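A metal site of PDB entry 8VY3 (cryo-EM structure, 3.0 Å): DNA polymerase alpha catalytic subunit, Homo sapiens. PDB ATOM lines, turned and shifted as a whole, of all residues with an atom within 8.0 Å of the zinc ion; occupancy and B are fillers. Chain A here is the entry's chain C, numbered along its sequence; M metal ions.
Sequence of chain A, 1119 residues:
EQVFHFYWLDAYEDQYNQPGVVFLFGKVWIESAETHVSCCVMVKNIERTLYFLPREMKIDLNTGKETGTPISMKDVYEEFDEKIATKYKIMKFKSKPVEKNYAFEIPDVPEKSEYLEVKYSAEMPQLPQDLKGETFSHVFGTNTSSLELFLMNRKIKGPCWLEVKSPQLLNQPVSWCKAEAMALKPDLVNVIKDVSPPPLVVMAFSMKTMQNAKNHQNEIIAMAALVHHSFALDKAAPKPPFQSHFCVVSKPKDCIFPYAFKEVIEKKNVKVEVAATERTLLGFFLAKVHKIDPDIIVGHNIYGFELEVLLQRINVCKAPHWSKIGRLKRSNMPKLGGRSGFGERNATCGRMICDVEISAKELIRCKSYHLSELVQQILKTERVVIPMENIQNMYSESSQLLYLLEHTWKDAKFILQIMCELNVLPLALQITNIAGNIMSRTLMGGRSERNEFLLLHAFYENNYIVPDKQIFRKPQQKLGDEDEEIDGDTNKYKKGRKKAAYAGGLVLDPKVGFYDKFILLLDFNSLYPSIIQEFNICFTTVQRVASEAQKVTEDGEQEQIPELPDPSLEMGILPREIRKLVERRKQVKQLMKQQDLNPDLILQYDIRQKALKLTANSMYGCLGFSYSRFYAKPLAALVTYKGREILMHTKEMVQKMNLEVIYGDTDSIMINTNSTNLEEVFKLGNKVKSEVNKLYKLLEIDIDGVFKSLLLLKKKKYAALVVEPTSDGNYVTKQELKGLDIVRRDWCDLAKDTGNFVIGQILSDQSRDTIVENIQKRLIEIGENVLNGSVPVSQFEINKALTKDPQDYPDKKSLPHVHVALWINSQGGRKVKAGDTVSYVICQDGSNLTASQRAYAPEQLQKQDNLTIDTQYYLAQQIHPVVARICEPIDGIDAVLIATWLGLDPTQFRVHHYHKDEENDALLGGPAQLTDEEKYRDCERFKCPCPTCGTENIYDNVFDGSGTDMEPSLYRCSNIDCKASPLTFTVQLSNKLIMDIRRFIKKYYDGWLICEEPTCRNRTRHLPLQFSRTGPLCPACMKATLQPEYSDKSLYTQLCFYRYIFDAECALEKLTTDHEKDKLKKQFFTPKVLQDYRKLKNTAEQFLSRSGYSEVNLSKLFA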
ATOM      1  N   VAL A 743      17.661   6.644  -9.434  1.00  0.00           N
ATOM      2  CA  VAL A 743      18.779   7.125  -8.623  1.00  0.00           C
ATOM      3  C   VAL A 743      19.496   8.263  -9.337  1.00  0.00           C
ATOM      4  O   VAL A 743      19.855   9.270  -8.712  1.00  0.00           O
ATOM      5  CB  VAL A 743      19.745   5.983  -8.289  1.00  0.00           C
ATOM      6  CG1 VAL A 743      20.982   6.512  -7.596  1.00  0.00           C
ATOM      7  CG2 VAL A 743      19.050   4.950  -7.406  1.00  0.00           C
ATOM      8  N   ILE A1010      26.600  -6.409 -15.622  1.00  0.00           N
ATOM      9  CA  ILE A1010      25.832  -5.237 -16.018  1.00  0.00           C
ATOM     10  C   ILE A1010      24.507  -5.255 -15.277  1.00  0.00           C
ATOM     11  O   ILE A1010      23.881  -6.311 -15.124  1.00  0.00           O
ATOM     12  CB  ILE A1010      25.630  -5.167 -17.543  1.00  0.00           C
ATOM     13  CG1 ILE A1010      24.962  -3.854 -17.937  1.00  0.00           C
ATOM     14  CG2 ILE A1010      24.846  -6.371 -18.044  1.00  0.00           C
ATOM     15  CD1 ILE A1010      24.876  -3.656 -19.424  1.00  0.00           C
ATOM     16  N   CYS A1011      24.090  -4.092 -14.766  1.00  0.00           N
ATOM     17  CA  CYS A1011      22.884  -4.009 -13.962  1.00  0.00           C
ATOM     18  C   CYS A1011      21.649  -4.258 -14.820  1.00  0.00           C
ATOM     19  O   CYS A1011      21.648  -4.038 -16.030  1.00  0.00           O
ATOM     20  CB  CYS A1011      22.799  -2.632 -13.293  1.00  0.00           C
ATOM     21  SG  CYS A1011      21.278  -2.336 -12.393  1.00  0.00           S
ATOM     22  N   GLU A1012      20.586  -4.730 -14.174  1.00  0.00           N
ATOM     23  CA  GLU A1012      19.389  -5.153 -14.890  1.00  0.00           C
ATOM     24  C   GLU A1012      18.397  -4.002 -15.081  1.00  0.00           C
ATOM     25  O   GLU A1012      17.501  -4.096 -15.928  1.00  0.00           O
ATOM     26  CB  GLU A1012      18.718  -6.316 -14.161  1.00  0.00           C
ATOM     27  CG  GLU A1012      17.753  -5.871 -13.071  1.00  0.00           C
ATOM     28  CD  GLU A1012      17.228  -7.024 -12.247  1.00  0.00           C
ATOM     29  OE1 GLU A1012      17.228  -8.160 -12.751  1.00  0.00           O
ATOM     30  OE2 GLU A1012      16.802  -6.788 -11.095  1.00  0.00           O
ATOM     31  N   GLU A1013      18.534  -2.935 -14.317  1.00  0.00           N
ATOM     32  CA  GLU A1013      17.622  -1.804 -14.403  1.00  0.00           C
ATOM     33  C   GLU A1013      17.937  -0.971 -15.647  1.00  0.00           C
ATOM     34  O   GLU A1013      19.082  -0.565 -15.837  1.00  0.00           O
ATOM     35  CB  GLU A1013      17.739  -0.949 -13.156  1.00  0.00           C
ATOM     36  CG  GLU A1013      16.527  -0.081 -12.865  1.00  0.00           C
ATOM     37  CD  GLU A1013      16.784   0.923 -11.761  1.00  0.00           C
ATOM     38  OE1 GLU A1013      16.743   2.139 -12.046  1.00  0.00           O
ATOM     39  OE2 GLU A1013      17.025   0.509 -10.609  1.00  0.00           O
ATOM     40  N   PRO A1014      16.939  -0.699 -16.505  1.00  0.00           N
ATOM     41  CA  PRO A1014      17.220   0.064 -17.734  1.00  0.00           C
ATOM     42  C   PRO A1014      17.781   1.451 -17.484  1.00  0.00           C
ATOM     43  O   PRO A1014      18.557   1.954 -18.311  1.00  0.00           O
ATOM     44  CB  PRO A1014      15.857   0.131 -18.420  1.00  0.00           C
ATOM     45  CG  PRO A1014      15.114  -1.030 -17.877  1.00  0.00           C
ATOM     46  CD  PRO A1014      15.540  -1.143 -16.453  1.00  0.00           C
ATOM     47  N   THR A1015      17.414   2.101 -16.385  1.00  0.00           N
ATOM     48  CA  THR A1015      17.911   3.427 -16.086  1.00  0.00           C
ATOM     49  C   THR A1015      19.277   3.425 -15.397  1.00  0.00           C
ATOM     50  O   THR A1015      19.916   4.470 -15.343  1.00  0.00           O
ATOM     51  CB  THR A1015      16.906   4.184 -15.218  1.00  0.00           C
ATOM     52  OG1 THR A1015      16.642   3.441 -14.020  1.00  0.00           O
ATOM     53  CG2 THR A1015      15.607   4.400 -15.961  1.00  0.00           C
ATOM     54  N   CYS A1016      19.730   2.285 -14.874  1.00  0.00           N
ATOM     55  CA  CYS A1016      21.046   2.229 -14.256  1.00  0.00           C
ATOM     56  C   CYS A1016      22.102   1.731 -15.230  1.00  0.00           C
ATOM     57  O   CYS A1016      23.009   2.480 -15.598  1.00  0.00           O
ATOM     58  CB  CYS A1016      21.007   1.331 -13.017  1.00  0.00           C
ATOM     59  SG  CYS A1016      22.594   1.119 -12.195  1.00  0.00           S
ATOM     60  N   ARG A1017      21.960   0.478 -15.679  1.00  0.00           N
ATOM     61  CA  ARG A1017      22.910  -0.158 -16.605  1.00  0.00           C
ATOM     62  C   ARG A1017      24.360   0.036 -16.166  1.00  0.00           C
ATOM     63  O   ARG A1017      25.211   0.428 -16.974  1.00  0.00           O
ATOM     64  CB  ARG A1017      22.696   0.345 -18.036  1.00  0.00           C
ATOM     65  CG  ARG A1017      21.381  -0.096 -18.637  1.00  0.00           C
ATOM     66  CD  ARG A1017      21.484  -1.486 -19.234  1.00  0.00           C
ATOM     67  NE  ARG A1017      20.461  -2.388 -18.721  1.00  0.00           N
ATOM     68  CZ  ARG A1017      19.408  -2.801 -19.415  1.00  0.00           C
ATOM     69  NH1 ARG A1017      19.196  -2.395 -20.652  1.00  0.00           N
ATOM     70  NH2 ARG A1017      18.541  -3.636 -18.841  1.00  0.00           N
ATOM     71  N   ASN A1018      24.644  -0.230 -14.901  1.00  0.00           N
ATOM     72  CA  ASN A1018      26.004  -0.080 -14.383  1.00  0.00           C
ATOM     73  C   ASN A1018      26.868  -1.256 -14.825  1.00  0.00           C
ATOM     74  O   ASN A1018      26.484  -2.417 -14.665  1.00  0.00           O
ATOM     75  CB  ASN A1018      25.961   0.012 -12.857  1.00  0.00           C
ATOM     76  CG  ASN A1018      27.337   0.173 -12.243  1.00  0.00           C
ATOM     77  OD1 ASN A1018      28.155   0.949 -12.716  1.00  0.00           O
ATOM     78  ND2 ASN A1018      27.601  -0.587 -11.184  1.00  0.00           N
ATOM     79  N   ARG A1019      28.039  -0.954 -15.366  1.00  0.00           N
ATOM     80  CA  ARG A1019      28.952  -1.965 -15.915  1.00  0.00           C
ATOM     81  C   ARG A1019      30.167  -2.056 -15.009  1.00  0.00           C
ATOM     82  O   ARG A1019      30.821  -1.049 -14.737  1.00  0.00           O
ATOM     83  CB  ARG A1019      29.345  -1.593 -17.344  1.00  0.00           C
ATOM     84  CG  ARG A1019      29.256  -2.714 -18.349  1.00  0.00           C
ATOM     85  CD  ARG A1019      30.134  -2.380 -19.544  1.00  0.00           C
ATOM     86  NE  ARG A1019      30.538  -3.561 -20.297  1.00  0.00           N
ATOM     87  CZ  ARG A1019      31.625  -3.614 -21.057  1.00  0.00           C
ATOM     88  NH1 ARG A1019      32.437  -2.577 -21.182  1.00  0.00           N
ATOM     89  NH2 ARG A1019      31.891  -4.729 -21.726  1.00  0.00           N
ATOM     90  N   LEU A1033      24.283  -7.635  -5.704  1.00  0.00           N
ATOM     91  CA  LEU A1033      23.500  -6.414  -5.556  1.00  0.00           C
ATOM     92  C   LEU A1033      24.314  -5.250  -6.099  1.00  0.00           C
ATOM     93  O   LEU A1033      25.484  -5.081  -5.755  1.00  0.00           O
ATOM     94  CB  LEU A1033      23.129  -6.207  -4.087  1.00  0.00           C
ATOM     95  CG  LEU A1033      22.326  -4.958  -3.735  1.00  0.00           C
ATOM     96  CD1 LEU A1033      20.880  -5.180  -4.114  1.00  0.00           C
ATOM     97  CD2 LEU A1033      22.448  -4.665  -2.257  1.00  0.00           C
ATOM     98  N   CYS A1034      23.689  -4.453  -6.964  1.00  0.00           N
ATOM     99  CA  CYS A1034      24.358  -3.353  -7.660  1.00  0.00           C
ATOM    100  C   CYS A1034      24.830  -2.281  -6.683  1.00  0.00           C
ATOM    101  O   CYS A1034      24.049  -1.813  -5.852  1.00  0.00           O
ATOM    102  CB  CYS A1034      23.422  -2.746  -8.704  1.00  0.00           C
ATOM    103  SG  CYS A1034      24.132  -1.421  -9.693  1.00  0.00           S
ATOM    104  N   PRO A1035      26.098  -1.893  -6.741  1.00  0.00           N
ATOM    105  CA  PRO A1035      26.615  -0.843  -5.835  1.00  0.00           C
ATOM    106  C   PRO A1035      26.309   0.593  -6.249  1.00  0.00           C
ATOM    107  O   PRO A1035      26.486   1.490  -5.406  1.00  0.00           O
ATOM    108  CB  PRO A1035      28.123  -1.102  -5.905  1.00  0.00           C
ATOM    109  CG  PRO A1035      28.332  -1.601  -7.283  1.00  0.00           C
ATOM    110  CD  PRO A1035      27.193  -2.540  -7.476  1.00  0.00           C
ATOM    111  N   ALA A1036      25.856   0.848  -7.474  1.00  0.00           N
ATOM    112  CA  ALA A1036      25.494   2.205  -7.869  1.00  0.00           C
ATOM    113  C   ALA A1036      24.083   2.524  -7.401  1.00  0.00           C
ATOM    114  O   ALA A1036      23.863   3.427  -6.587  1.00  0.00           O
ATOM    115  CB  ALA A1036      25.606   2.386  -9.383  1.00  0.00           C
ATOM    116  N   CYS A1037      23.096   1.785  -7.915  1.00  0.00           N
ATOM    117  CA  CYS A1037      21.759   1.792  -7.351  1.00  0.00           C
ATOM    118  C   CYS A1037      21.617   0.583  -6.442  1.00  0.00           C
ATOM    119  O   CYS A1037      21.789  -0.556  -6.894  1.00  0.00           O
ATOM    120  CB  CYS A1037      20.699   1.781  -8.451  1.00  0.00           C
ATOM    121  SG  CYS A1037      20.616   0.291  -9.469  1.00  0.00           S
ATOM    122  N   MET A1038      21.326   0.814  -5.170  1.00  0.00           N
ATOM    123  CA  MET A1038      21.452  -0.263  -4.202  1.00  0.00           C
ATOM    124  C   MET A1038      20.271  -1.224  -4.266  1.00  0.00           C
ATOM    125  O   MET A1038      20.156  -2.116  -3.407  1.00  0.00           O
ATOM    126  CB  MET A1038      21.609   0.315  -2.799  1.00  0.00           C
ATOM    127  CG  MET A1038      22.960   0.963  -2.551  1.00  0.00           C
ATOM    128  SD  MET A1038      24.289  -0.221  -2.239  1.00  0.00           S
ATOM    129  CE  MET A1038      23.461  -1.367  -1.149  1.00  0.00           C
ATOM    130  N   LYS A1039      19.387  -1.073  -5.253  1.00  0.00           N
ATOM    131  CA  LYS A1039      18.247  -1.956  -5.388  1.00  0.00           C
ATOM    132  C   LYS A1039      18.166  -2.477  -6.832  1.00  0.00           C
ATOM    133  O   LYS A1039      17.364  -2.045  -7.647  1.00  0.00           O
ATOM    134  CB  LYS A1039      16.961  -1.238  -4.961  1.00  0.00           C
ATOM    135  CG  LYS A1039      16.685   0.066  -5.701  1.00  0.00           C
ATOM    136  CD  LYS A1039      16.449   1.230  -4.742  1.00  0.00           C
ATOM    137  CE  LYS A1039      15.944   2.443  -5.495  1.00  0.00           C
ATOM    138  NZ  LYS A1039      16.251   3.717  -4.784  1.00  0.00           N
ATOM    139  N   ALA A1040      18.984  -3.485  -7.117  1.00  0.00           N
ATOM    140  CA  ALA A1040      19.023  -4.149  -8.414  1.00  0.00           C
ATOM    141  C   ALA A1040      20.050  -5.269  -8.366  1.00  0.00           C
ATOM    142  O   ALA A1040      20.873  -5.320  -7.448  1.00  0.00           O
ATOM    143  CB  ALA A1040      19.362  -3.174  -9.534  1.00  0.00           C
ATOM    144  N   THR A1041      20.033  -6.160  -9.351  1.00  0.00           N
ATOM    145  CA  THR A1041      21.006  -7.246  -9.403  1.00  0.00           C
ATOM    146  C   THR A1041      21.827  -7.168 -10.685  1.00  0.00           C
ATOM    147  O   THR A1041      21.299  -6.928 -11.769  1.00  0.00           O
ATOM    148  CB  THR A1041      20.331  -8.610  -9.315  1.00  0.00           C
ATOM    149  OG1 THR A1041      19.537  -8.846 -10.482  1.00  0.00           O
ATOM    150  CG2 THR A1041      19.441  -8.688  -8.096  1.00  0.00           C
ATOM    151  N   LEU A1042      23.136  -7.374 -10.550  1.00  0.00           N
ATOM    152  CA  LEU A1042      24.030  -7.476 -11.681  1.00  0.00           C
ATOM    153  C   LEU A1042      23.872  -8.826 -12.354  1.00  0.00           C
ATOM    154  O   LEU A1042      23.481  -9.806 -11.707  1.00  0.00           O
ATOM    155  CB  LEU A1042      25.486  -7.276 -11.247  1.00  0.00           C
ATOM    156  CG  LEU A1042      25.788  -6.106 -10.322  1.00  0.00           C
ATOM    157  CD1 LEU A1042      27.158  -6.266  -9.714  1.00  0.00           C
ATOM    158  CD2 LEU A1042      25.711  -4.805 -11.072  1.00  0.00           C
HETATM  159 ZN    ZN M   1      22.336  -0.836 -11.001  1.00  0.00          ZN
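Within 4 Å of the zinc ion: Cys 1011, Cys 1016, Cys 1034 and Cys 1037.
N of Cys 1034 lies within hydrogen-bond range of O of Ala 1040, 3.0 Å away. The side-chain sulfur of Cys 1034 lies close to the backbone NH of Ala 1036, at 3.6 Å. The backbone NH of Cys 1011 is in hydrogen-bond range of the backbone carbonyl oxygen of Asn 1018, 2.9 Å away. The backbone carbonyl oxygen (O) of Cys 1011 sits at hydrogen-bond distance from the guanidinium group (NE) of Arg 1017 (3.4 Å). The side-chain sulfur (SG) of Cys 1011 sits close to the backbone NH (N) of Glu 1013 (3.4 Å). The side-chain sulfur of Cys 1016 sits close to the backbone NH of Asn 1018 (3.7 Å). The side-chain carboxylate (OE2) of Glu 1013 lies close to the side-chain sulfur (SG) of Cys 1037, at 3.8 Å.
The zinc ion is bound by SG of Cys 1034, SG of Cys 1011, SG of Cys 1016 and SG of Cys 1037.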
